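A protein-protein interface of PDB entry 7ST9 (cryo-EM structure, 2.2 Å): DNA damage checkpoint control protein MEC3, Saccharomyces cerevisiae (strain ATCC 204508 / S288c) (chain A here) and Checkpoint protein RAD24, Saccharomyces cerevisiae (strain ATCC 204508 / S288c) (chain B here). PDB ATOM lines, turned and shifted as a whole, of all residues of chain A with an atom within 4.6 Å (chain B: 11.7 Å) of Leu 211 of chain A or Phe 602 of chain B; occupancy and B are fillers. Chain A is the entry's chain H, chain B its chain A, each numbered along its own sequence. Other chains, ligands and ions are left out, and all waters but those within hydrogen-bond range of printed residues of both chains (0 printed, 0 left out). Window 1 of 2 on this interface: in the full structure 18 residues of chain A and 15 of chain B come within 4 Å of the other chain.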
ATOM      1  N   THR A  92       8.520  -2.648   6.878  1.00  0.00           N
ATOM      2  CA  THR A  92       9.617  -3.482   7.352  1.00  0.00           C
ATOM      3  C   THR A  92      10.198  -4.275   6.188  1.00  0.00           C
ATOM      4  O   THR A  92       9.451  -4.839   5.382  1.00  0.00           O
ATOM      5  CB  THR A  92       9.145  -4.435   8.452  1.00  0.00           C
ATOM      6  OG1 THR A  92       8.279  -3.734   9.353  1.00  0.00           O
ATOM      7  CG2 THR A  92      10.333  -4.993   9.222  1.00  0.00           C
ATOM      8  N   MET A  93      11.527  -4.315   6.108  1.00  0.00           N
ATOM      9  CA  MET A  93      12.221  -5.075   5.080  1.00  0.00           C
ATOM     10  C   MET A  93      13.412  -5.786   5.704  1.00  0.00           C
ATOM     11  O   MET A  93      13.905  -5.398   6.764  1.00  0.00           O
ATOM     12  CB  MET A  93      12.693  -4.175   3.930  1.00  0.00           C
ATOM     13  CG  MET A  93      11.565  -3.547   3.127  1.00  0.00           C
ATOM     14  SD  MET A  93      11.503  -1.751   3.287  1.00  0.00           S
ATOM     15  CE  MET A  93      13.058  -1.291   2.525  1.00  0.00           C
ATOM     16  N   LEU A 123      11.599   1.782  -3.835  1.00  0.00           N
ATOM     17  CA  LEU A 123      11.175   0.389  -3.778  1.00  0.00           C
ATOM     18  C   LEU A 123      10.462   0.045  -5.080  1.00  0.00           C
ATOM     19  O   LEU A 123       9.494   0.715  -5.456  1.00  0.00           O
ATOM     20  CB  LEU A 123      10.257   0.150  -2.578  1.00  0.00           C
ATOM     21  CG  LEU A 123       9.952  -1.308  -2.232  1.00  0.00           C
ATOM     22  CD1 LEU A 123      11.202  -2.026  -1.745  1.00  0.00           C
ATOM     23  CD2 LEU A 123       8.848  -1.386  -1.189  1.00  0.00           C
ATOM     24  N   ASN A 151       5.648 -13.478   1.521  1.00  0.00           N
ATOM     25  CA  ASN A 151       6.718 -12.487   1.573  1.00  0.00           C
ATOM     26  C   ASN A 151       7.339 -12.289   0.195  1.00  0.00           C
ATOM     27  O   ASN A 151       8.416 -12.816  -0.084  1.00  0.00           O
ATOM     28  CB  ASN A 151       7.791 -12.911   2.578  1.00  0.00           C
ATOM     29  CG  ASN A 151       8.084 -14.397   2.526  1.00  0.00           C
ATOM     30  OD1 ASN A 151       7.878 -15.047   1.501  1.00  0.00           O
ATOM     31  ND2 ASN A 151       8.569 -14.943   3.635  1.00  0.00           N
ATOM     32  N   PRO A 152       6.661 -11.536  -0.671  1.00  0.00           N
ATOM     33  CA  PRO A 152       7.215 -11.273  -2.004  1.00  0.00           C
ATOM     34  C   PRO A 152       8.530 -10.513  -1.922  1.00  0.00           C
ATOM     35  O   PRO A 152       8.754  -9.708  -1.015  1.00  0.00           O
ATOM     36  CB  PRO A 152       6.125 -10.437  -2.687  1.00  0.00           C
ATOM     37  CG  PRO A 152       4.878 -10.712  -1.913  1.00  0.00           C
ATOM     38  CD  PRO A 152       5.318 -10.955  -0.505  1.00  0.00           C
ATOM     39  N   CYS A 154      11.121  -7.841  -3.516  1.00  0.00           N
ATOM     40  CA  CYS A 154      11.178  -6.638  -4.336  1.00  0.00           C
ATOM     41  C   CYS A 154      12.638  -6.202  -4.474  1.00  0.00           C
ATOM     42  O   CYS A 154      13.559  -6.894  -4.031  1.00  0.00           O
ATOM     43  CB  CYS A 154      10.308  -5.538  -3.725  1.00  0.00           C
ATOM     44  SG  CYS A 154       8.841  -6.148  -2.863  1.00  0.00           S
ATOM     45  N   VAL A 209      15.300  -7.476  -1.793  1.00  0.00           N
ATOM     46  CA  VAL A 209      14.777  -7.134  -0.476  1.00  0.00           C
ATOM     47  C   VAL A 209      13.507  -7.939  -0.242  1.00  0.00           C
ATOM     48  O   VAL A 209      12.768  -8.251  -1.180  1.00  0.00           O
ATOM     49  CB  VAL A 209      14.513  -5.613  -0.359  1.00  0.00           C
ATOM     50  CG1 VAL A 209      13.529  -5.317   0.760  1.00  0.00           C
ATOM     51  CG2 VAL A 209      15.819  -4.864  -0.140  1.00  0.00           C
ATOM     52  N   LYS A 210      13.258  -8.281   1.020  1.00  0.00           N
ATOM     53  CA  LYS A 210      12.078  -9.039   1.417  1.00  0.00           C
ATOM     54  C   LYS A 210      11.297  -8.247   2.454  1.00  0.00           C
ATOM     55  O   LYS A 210      11.859  -7.821   3.468  1.00  0.00           O
ATOM     56  CB  LYS A 210      12.468 -10.408   1.981  1.00  0.00           C
ATOM     57  CG  LYS A 210      11.281 -11.303   2.301  1.00  0.00           C
ATOM     58  CD  LYS A 210      11.728 -12.680   2.763  1.00  0.00           C
ATOM     59  CE  LYS A 210      12.082 -12.680   4.241  1.00  0.00           C
ATOM     60  NZ  LYS A 210      12.460 -14.037   4.724  1.00  0.00           N
ATOM     61  N   LEU A 211      10.006  -8.055   2.199  1.00  0.00           N
ATOM     62  CA  LEU A 211       9.148  -7.335   3.126  1.00  0.00           C
ATOM     63  C   LEU A 211       8.644  -8.267   4.225  1.00  0.00           C
ATOM     64  O   LEU A 211       8.570  -9.488   4.060  1.00  0.00           O
ATOM     65  CB  LEU A 211       7.965  -6.707   2.387  1.00  0.00           C
ATOM     66  CG  LEU A 211       8.217  -5.320   1.789  1.00  0.00           C
ATOM     67  CD1 LEU A 211       9.385  -5.351   0.816  1.00  0.00           C
ATOM     68  CD2 LEU A 211       6.963  -4.795   1.107  1.00  0.00           C
ATOM     69  N   LEU A 212       8.295  -7.669   5.361  1.00  0.00           N
ATOM     70  CA  LEU A 212       7.835  -8.403   6.530  1.00  0.00           C
ATOM     71  C   LEU A 212       6.425  -7.962   6.902  1.00  0.00           C
ATOM     72  O   LEU A 212       6.051  -6.800   6.721  1.00  0.00           O
ATOM     73  CB  LEU A 212       8.775  -8.192   7.724  1.00  0.00           C
ATOM     74  CG  LEU A 212       9.901  -9.216   7.877  1.00  0.00           C
ATOM     75  CD1 LEU A 212      10.876  -9.124   6.713  1.00  0.00           C
ATOM     76  CD2 LEU A 212      10.622  -9.023   9.201  1.00  0.00           C
ATOM     77  N   PHE A 213       5.647  -8.908   7.424  1.00  0.00           N
ATOM     78  CA  PHE A 213       4.282  -8.634   7.841  1.00  0.00           C
ATOM     79  C   PHE A 213       4.263  -8.019   9.240  1.00  0.00           C
ATOM     80  O   PHE A 213       5.285  -7.929   9.927  1.00  0.00           O
ATOM     81  CB  PHE A 213       3.449  -9.916   7.818  1.00  0.00           C
ATOM     82  CG  PHE A 213       3.345 -10.550   6.458  1.00  0.00           C
ATOM     83  CD1 PHE A 213       4.411 -11.256   5.922  1.00  0.00           C
ATOM     84  CD2 PHE A 213       2.179 -10.446   5.720  1.00  0.00           C
ATOM     85  CE1 PHE A 213       4.316 -11.840   4.673  1.00  0.00           C
ATOM     86  CE2 PHE A 213       2.079 -11.029   4.470  1.00  0.00           C
ATOM     87  CZ  PHE A 213       3.148 -11.727   3.948  1.00  0.00           C
ATOM     88  N   VAL B 588      16.735 -19.725   0.133  1.00  0.00           N
ATOM     89  CA  VAL B 588      16.436 -19.078   1.453  1.00  0.00           C
ATOM     90  C   VAL B 588      15.815 -17.694   1.194  1.00  0.00           C
ATOM     91  O   VAL B 588      14.695 -17.430   1.692  1.00  0.00           O
ATOM     92  CB  VAL B 588      17.684 -18.978   2.366  1.00  0.00           C
ATOM     93  CG1 VAL B 588      17.370 -18.235   3.678  1.00  0.00           C
ATOM     94  CG2 VAL B 588      18.283 -20.365   2.661  1.00  0.00           C
ATOM     95  N   MET B 589      16.504 -16.834   0.436  1.00  0.00           N
ATOM     96  CA  MET B 589      16.066 -15.432   0.173  1.00  0.00           C
ATOM     97  C   MET B 589      14.813 -15.477  -0.714  1.00  0.00           C
ATOM     98  O   MET B 589      13.913 -14.632  -0.510  1.00  0.00           O
ATOM     99  CB  MET B 589      17.159 -14.600  -0.522  1.00  0.00           C
ATOM    100  CG  MET B 589      16.750 -13.133  -0.822  1.00  0.00           C
ATOM    101  SD  MET B 589      16.316 -12.204   0.676  1.00  0.00           S
ATOM    102  CE  MET B 589      15.689 -10.679  -0.028  1.00  0.00           C
ATOM    103  N   MET B 590      14.739 -16.425  -1.658  1.00  0.00           N
ATOM    104  CA  MET B 590      13.603 -16.523  -2.622  1.00  0.00           C
ATOM    105  C   MET B 590      12.290 -16.641  -1.832  1.00  0.00           C
ATOM    106  O   MET B 590      11.330 -15.915  -2.180  1.00  0.00           O
ATOM    107  CB  MET B 590      13.747 -17.727  -3.570  1.00  0.00           C
ATOM    108  CG  MET B 590      12.617 -17.840  -4.624  1.00  0.00           C
ATOM    109  SD  MET B 590      11.204 -18.813  -4.032  1.00  0.00           S
ATOM    110  CE  MET B 590       9.981 -18.440  -5.286  1.00  0.00           C
ATOM    111  N   ALA B 591      12.222 -17.523  -0.826  1.00  0.00           N
ATOM    112  CA  ALA B 591      11.013 -17.705   0.023  1.00  0.00           C
ATOM    113  C   ALA B 591      11.343 -18.496   1.299  1.00  0.00           C
ATOM    114  O   ALA B 591      12.261 -19.336   1.226  1.00  0.00           O
ATOM    115  CB  ALA B 591       9.916 -18.410  -0.766  1.00  0.00           C
ATOM    116  N   ASN B 592      10.627 -18.259   2.408  1.00  0.00           N
ATOM    117  CA  ASN B 592      10.800 -19.007   3.689  1.00  0.00           C
ATOM    118  C   ASN B 592       9.408 -19.386   4.220  1.00  0.00           C
ATOM    119  O   ASN B 592       8.476 -18.580   4.020  1.00  0.00           O
ATOM    120  CB  ASN B 592      11.599 -18.202   4.728  1.00  0.00           C
ATOM    121  CG  ASN B 592      13.084 -18.114   4.420  1.00  0.00           C
ATOM    122  OD1 ASN B 592      13.679 -19.073   3.930  1.00  0.00           O
ATOM    123  ND2 ASN B 592      13.716 -16.990   4.726  1.00  0.00           N
ATOM    124  N   ASP B 593       9.265 -20.545   4.877  1.00  0.00           N
ATOM    125  CA  ASP B 593       7.955 -21.025   5.406  1.00  0.00           C
ATOM    126  C   ASP B 593       7.462 -20.023   6.461  1.00  0.00           C
ATOM    127  O   ASP B 593       6.252 -19.691   6.444  1.00  0.00           O
ATOM    128  CB  ASP B 593       8.041 -22.443   5.994  1.00  0.00           C
ATOM    129  CG  ASP B 593       8.401 -23.530   4.985  1.00  0.00           C
ATOM    130  OD1 ASP B 593       8.527 -23.205   3.786  1.00  0.00           O
ATOM    131  OD2 ASP B 593       8.553 -24.702   5.402  1.00  0.00           O
ATOM    132  N   ASP B 594       8.351 -19.557   7.349  1.00  0.00           N
ATOM    133  CA  ASP B 594       7.981 -18.605   8.441  1.00  0.00           C
ATOM    134  C   ASP B 594       6.673 -19.116   9.076  1.00  0.00           C
ATOM    135  O   ASP B 594       6.667 -20.302   9.481  1.00  0.00           O
ATOM    136  CB  ASP B 594       7.956 -17.162   7.903  1.00  0.00           C
ATOM    137  CG  ASP B 594       9.301 -16.650   7.394  1.00  0.00           C
ATOM    138  OD1 ASP B 594      10.325 -17.314   7.660  1.00  0.00           O
ATOM    139  OD2 ASP B 594       9.325 -15.580   6.742  1.00  0.00           O
ATOM    140  N   LEU B 595       5.613 -18.295   9.179  1.00  0.00           N
ATOM    141  CA  LEU B 595       4.306 -18.675   9.793  1.00  0.00           C
ATOM    142  C   LEU B 595       3.159 -18.303   8.843  1.00  0.00           C
ATOM    143  O   LEU B 595       3.456 -17.698   7.792  1.00  0.00           O
ATOM    144  CB  LEU B 595       4.155 -17.942  11.138  1.00  0.00           C
ATOM    145  CG  LEU B 595       5.258 -18.193  12.179  1.00  0.00           C
ATOM    146  CD1 LEU B 595       5.137 -17.208  13.359  1.00  0.00           C
ATOM    147  CD2 LEU B 595       5.216 -19.646  12.688  1.00  0.00           C
ATOM    148  N   GLU B 596       1.905 -18.636   9.183  1.00  0.00           N
ATOM    149  CA  GLU B 596       0.740 -18.262   8.393  1.00  0.00           C
ATOM    150  C   GLU B 596       0.304 -16.855   8.785  1.00  0.00           C
ATOM    151  O   GLU B 596       0.044 -16.585   9.962  1.00  0.00           O
ATOM    152  CB  GLU B 596      -0.400 -19.258   8.600  1.00  0.00           C
ATOM    153  CG  GLU B 596      -0.908 -19.342  10.033  1.00  0.00           C
ATOM    154  CD  GLU B 596      -2.235 -18.632  10.226  1.00  0.00           C
ATOM    155  OE1 GLU B 596      -3.156 -18.855   9.411  1.00  0.00           O
ATOM    156  OE2 GLU B 596      -2.358 -17.853  11.194  1.00  0.00           O
ATOM    157  N   ASP B 597       0.230 -15.964   7.802  1.00  0.00           N
ATOM    158  CA  ASP B 597      -0.141 -14.573   8.014  1.00  0.00           C
ATOM    159  C   ASP B 597      -1.242 -14.185   7.026  1.00  0.00           C
ATOM    160  O   ASP B 597      -1.749 -15.015   6.267  1.00  0.00           O
ATOM    161  CB  ASP B 597       1.085 -13.667   7.877  1.00  0.00           C
ATOM    162  CG  ASP B 597       2.270 -14.167   8.680  1.00  0.00           C
ATOM    163  OD1 ASP B 597       2.231 -14.069   9.924  1.00  0.00           O
ATOM    164  OD2 ASP B 597       3.240 -14.658   8.067  1.00  0.00           O
ATOM    165  N   GLU B 598      -1.609 -12.902   7.042  1.00  0.00           N
ATOM    166  CA  GLU B 598      -2.644 -12.377   6.152  1.00  0.00           C
ATOM    167  C   GLU B 598      -1.988 -11.986   4.829  1.00  0.00           C
ATOM    168  O   GLU B 598      -1.761 -10.813   4.527  1.00  0.00           O
ATOM    169  CB  GLU B 598      -3.361 -11.199   6.798  1.00  0.00           C
ATOM    170  CG  GLU B 598      -4.148 -11.564   8.047  1.00  0.00           C
ATOM    171  CD  GLU B 598      -4.854 -10.370   8.660  1.00  0.00           C
ATOM    172  OE1 GLU B 598      -4.737  -9.259   8.104  1.00  0.00           O
ATOM    173  OE2 GLU B 598      -5.527 -10.545   9.698  1.00  0.00           O
ATOM    174  N   GLU B 599      -1.679 -13.007   4.026  1.00  0.00           N
ATOM    175  CA  GLU B 599      -1.050 -12.762   2.733  1.00  0.00           C
ATOM    176  C   GLU B 599      -1.975 -12.001   1.793  1.00  0.00           C
ATOM    177  O   GLU B 599      -1.505 -11.190   0.987  1.00  0.00           O
ATOM    178  CB  GLU B 599      -0.623 -14.086   2.098  1.00  0.00           C
ATOM    179  CG  GLU B 599       0.533 -14.767   2.811  1.00  0.00           C
ATOM    180  CD  GLU B 599       0.912 -16.089   2.175  1.00  0.00           C
ATOM    181  OE1 GLU B 599       0.161 -16.566   1.298  1.00  0.00           O
ATOM    182  OE2 GLU B 599       1.962 -16.653   2.551  1.00  0.00           O
ATOM    183  N   THR B 600      -3.284 -12.245   1.878  1.00  0.00           N
ATOM    184  CA  THR B 600      -4.222 -11.534   1.015  1.00  0.00           C
ATOM    185  C   THR B 600      -4.183 -10.033   1.277  1.00  0.00           C
ATOM    186  O   THR B 600      -4.201  -9.233   0.336  1.00  0.00           O
ATOM    187  CB  THR B 600      -5.639 -12.072   1.221  1.00  0.00           C
ATOM    188  OG1 THR B 600      -6.004 -11.952   2.601  1.00  0.00           O
ATOM    189  CG2 THR B 600      -5.723 -13.533   0.800  1.00  0.00           C
ATOM    190  N   SER B 601      -4.127  -9.633   2.550  1.00  0.00           N
ATOM    191  CA  SER B 601      -4.040  -8.214   2.872  1.00  0.00           C
ATOM    192  C   SER B 601      -2.755  -7.599   2.334  1.00  0.00           C
ATOM    193  O   SER B 601      -2.743  -6.424   1.949  1.00  0.00           O
ATOM    194  CB  SER B 601      -4.131  -8.012   4.384  1.00  0.00           C
ATOM    195  OG  SER B 601      -4.187  -6.635   4.712  1.00  0.00           O
ATOM    196  N   PHE B 602      -1.668  -8.372   2.301  1.00  0.00           N
ATOM    197  CA  PHE B 602      -0.413  -7.857   1.763  1.00  0.00           C
ATOM    198  C   PHE B 602      -0.560  -7.481   0.294  1.00  0.00           C
ATOM    199  O   PHE B 602      -0.057  -6.438  -0.142  1.00  0.00           O
ATOM    200  CB  PHE B 602       0.696  -8.892   1.943  1.00  0.00           C
ATOM    201  CG  PHE B 602       2.081  -8.325   1.819  1.00  0.00           C
ATOM    202  CD1 PHE B 602       2.684  -8.201   0.578  1.00  0.00           C
ATOM    203  CD2 PHE B 602       2.780  -7.916   2.942  1.00  0.00           C
ATOM    204  CE1 PHE B 602       3.959  -7.680   0.461  1.00  0.00           C
ATOM    205  CE2 PHE B 602       4.055  -7.395   2.830  1.00  0.00           C
ATOM    206  CZ  PHE B 602       4.644  -7.277   1.588  1.00  0.00           C
ATOM    207  N   ASN B 603      -1.243  -8.319  -0.487  1.00  0.00           N
ATOM    208  CA  ASN B 603      -1.474  -8.006  -1.891  1.00  0.00           C
ATOM    209  C   ASN B 603      -2.467  -6.866  -2.073  1.00  0.00           C
ATOM    210  O   ASN B 603      -2.510  -6.264  -3.151  1.00  0.00           O
ATOM    211  CB  ASN B 603      -1.972  -9.250  -2.630  1.00  0.00           C
ATOM    212  CG  ASN B 603      -1.875  -9.112  -4.137  1.00  0.00           C
ATOM    213  OD1 ASN B 603      -0.996  -8.421  -4.654  1.00  0.00           O
ATOM    214  ND2 ASN B 603      -2.779  -9.772  -4.851  1.00  0.00           N
ATOM    215  N   ASP B 604      -3.264  -6.558  -1.048  1.00  0.00           N
ATOM    216  CA  ASP B 604      -4.238  -5.477  -1.142  1.00  0.00           C
ATOM    217  C   ASP B 604      -3.598  -4.098  -1.069  1.00  0.00           C
ATOM    218  O   ASP B 604      -4.283  -3.103  -1.330  1.00  0.00           O
ATOM    219  CB  ASP B 604      -5.282  -5.618  -0.032  1.00  0.00           C
ATOM    220  CG  ASP B 604      -6.209  -6.799  -0.248  1.00  0.00           C
ATOM    221  OD1 ASP B 604      -6.262  -7.317  -1.383  1.00  0.00           O
ATOM    222  OD2 ASP B 604      -6.884  -7.210   0.719  1.00  0.00           O
ATOM    223  N   ASP B 605      -2.314  -4.012  -0.722  1.00  0.00           N
ATOM    224  CA  ASP B 605      -1.585  -2.745  -0.647  1.00  0.00           C
ATOM    225  C   ASP B 605      -0.317  -2.889  -1.477  1.00  0.00           C
ATOM    226  O   ASP B 605       0.788  -3.017  -0.933  1.00  0.00           O
ATOM    227  CB  ASP B 605      -1.270  -2.373   0.803  1.00  0.00           C
ATOM    228  CG  ASP B 605      -0.801  -3.558   1.625  1.00  0.00           C
ATOM    229  OD1 ASP B 605       0.157  -4.240   1.202  1.00  0.00           O
ATOM    230  OD2 ASP B 605      -1.391  -3.810   2.696  1.00  0.00           O
ATOM    231  N   PRO B 606      -0.436  -2.862  -2.803  1.00  0.00           N
ATOM    232  CA  PRO B 606       0.725  -3.113  -3.660  1.00  0.00           C
ATOM    233  C   PRO B 606       1.630  -1.901  -3.806  1.00  0.00           C
ATOM    234  O   PRO B 606       1.204  -0.747  -3.726  1.00  0.00           O
ATOM    235  CB  PRO B 606       0.089  -3.486  -5.009  1.00  0.00           C
ATOM    236  CG  PRO B 606      -1.365  -3.060  -4.929  1.00  0.00           C
ATOM    237  CD  PRO B 606      -1.609  -2.444  -3.586  1.00  0.00           C
ATOM    238  N   ILE B 607       2.912  -2.193  -4.021  1.00  0.00           N
ATOM    239  CA  ILE B 607       3.923  -1.166  -4.251  1.00  0.00           C
ATOM    240  C   ILE B 607       3.472  -0.273  -5.398  1.00  0.00           C
ATOM    241  O   ILE B 607       2.819  -0.734  -6.341  1.00  0.00           O
ATOM    242  CB  ILE B 607       5.306  -1.779  -4.555  1.00  0.00           C
ATOM    243  CG1 ILE B 607       5.210  -2.901  -5.600  1.00  0.00           C
ATOM    244  CG2 ILE B 607       5.942  -2.306  -3.278  1.00  0.00           C
ATOM    245  CD1 ILE B 607       5.441  -2.430  -7.019  1.00  0.00           C
ATOM    246  N   VAL B 608       3.812   1.012  -5.322  1.00  0.00           N
ATOM    247  CA  VAL B 608       3.540   1.968  -6.389  1.00  0.00           C
ATOM    248  C   VAL B 608       4.839   2.697  -6.698  1.00  0.00           C
ATOM    249  O   VAL B 608       5.405   3.362  -5.821  1.00  0.00           O
ATOM    250  CB  VAL B 608       2.435   2.966  -6.005  1.00  0.00           C
ATOM    251  CG1 VAL B 608       2.175   3.937  -7.148  1.00  0.00           C
ATOM    252  CG2 VAL B 608       1.161   2.227  -5.624  1.00  0.00           C
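ND2 of Asn 592 of chain B lies close to NZ of Lys 210 of chain A, at 3.2 Å. ND2 of Asn 151 of chain A lies within hydrogen-bond range of OD2 of Asp 594 of chain B (3.3 Å).
OD1 of Asn 592 of chain B lies close to O of Val 588 of chain B, at 3.0 Å. O of Phe 602 of chain B sits close to OD1 of Asp 605 of chain B, 2.6 Å away. The backbone carbonyl oxygen (O) of Val 209 of chain A is in hydrogen-bond range of the backbone NH (N) of Cys 154 of chain A (2.9 Å).
Of the printed residues of chain B, Leu 211 of chain A touches Phe 602. Of chain A, only Pro 152, Leu 211 and Phe 213 come within 4 Å of Phe 602 of chain B. No residue of chain B comes within 4 Å of Met 93 of chain A. Asn 151 of chain A touches two residues of chain B. Of chain B, only Phe 602 (3.7 Å) comes within 4 Å of Pro 152 of chain A. Lys 210 of chain A touches two residues of chain B. Phe 213 of chain A touches three residues of chain B. Printed residues of chain A within 4 Å of Asp 594 of chain B: Asn 151. Of the printed residues of chain A, Met 589 of chain B touches Val 209 (3.5 Å) and Lys 210 (3.6 Å). Printed residues of chain B within 4 Å of Leu 123 of chain A: Ile 607. Of the printed residues of chain A, Glu 599 of chain B touches Phe 213. Printed residues of chain A within 4 Å of Ile 607 of chain B: Leu 123 (3.7 Å). Leu 595 of chain B touches none of the printed residues of chain A. Pro 606 of chain B touches none of the printed residues of chain A. The nearest residue of chain B that does not touch Leu 211 of chain A is Ile 607 of chain B (5.1 Å). The nearest residue of chain A that does not touch Phe 602 of chain B is Leu 212 of chain A (4.4 Å). The nearest printed residue of chain A that does not touch Asn 592 of chain B is Phe 213 of chain A (7.9 Å).
Among the printed residues, pairs that only touch across the chains: Leu 123 of chain A with Ile 607 of chain B, Asn 151 of chain A with Asn 592 of chain B, Pro 152 of chain A with Phe 602 of chain B, Val 209 of chain A with Met 589 of chain B, Lys 210 of chain A with Met 589 of chain B, Leu 211 of chain A with Phe 602 of chain B, Phe 213 of chain A with Glu 598 of chain B, Phe 213 of chain A with Glu 599 of chain B and Phe 213 of chain A with Phe 602 of chain B.
Hydrophobic or aromatic side chains of chain B within 4 Å of the printed part of chain A: Met 589, Phe 602 and Ile 607. Of the 11 printed residues of chain A, 7 touch a printed residue of chain B. Hydrophobic or aromatic side chains of chain A that line the printed part of chain B: Leu 123, Pro 152, Leu 211 and Phe 213. Among the printed residues, 11 pairs touch across the chains.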
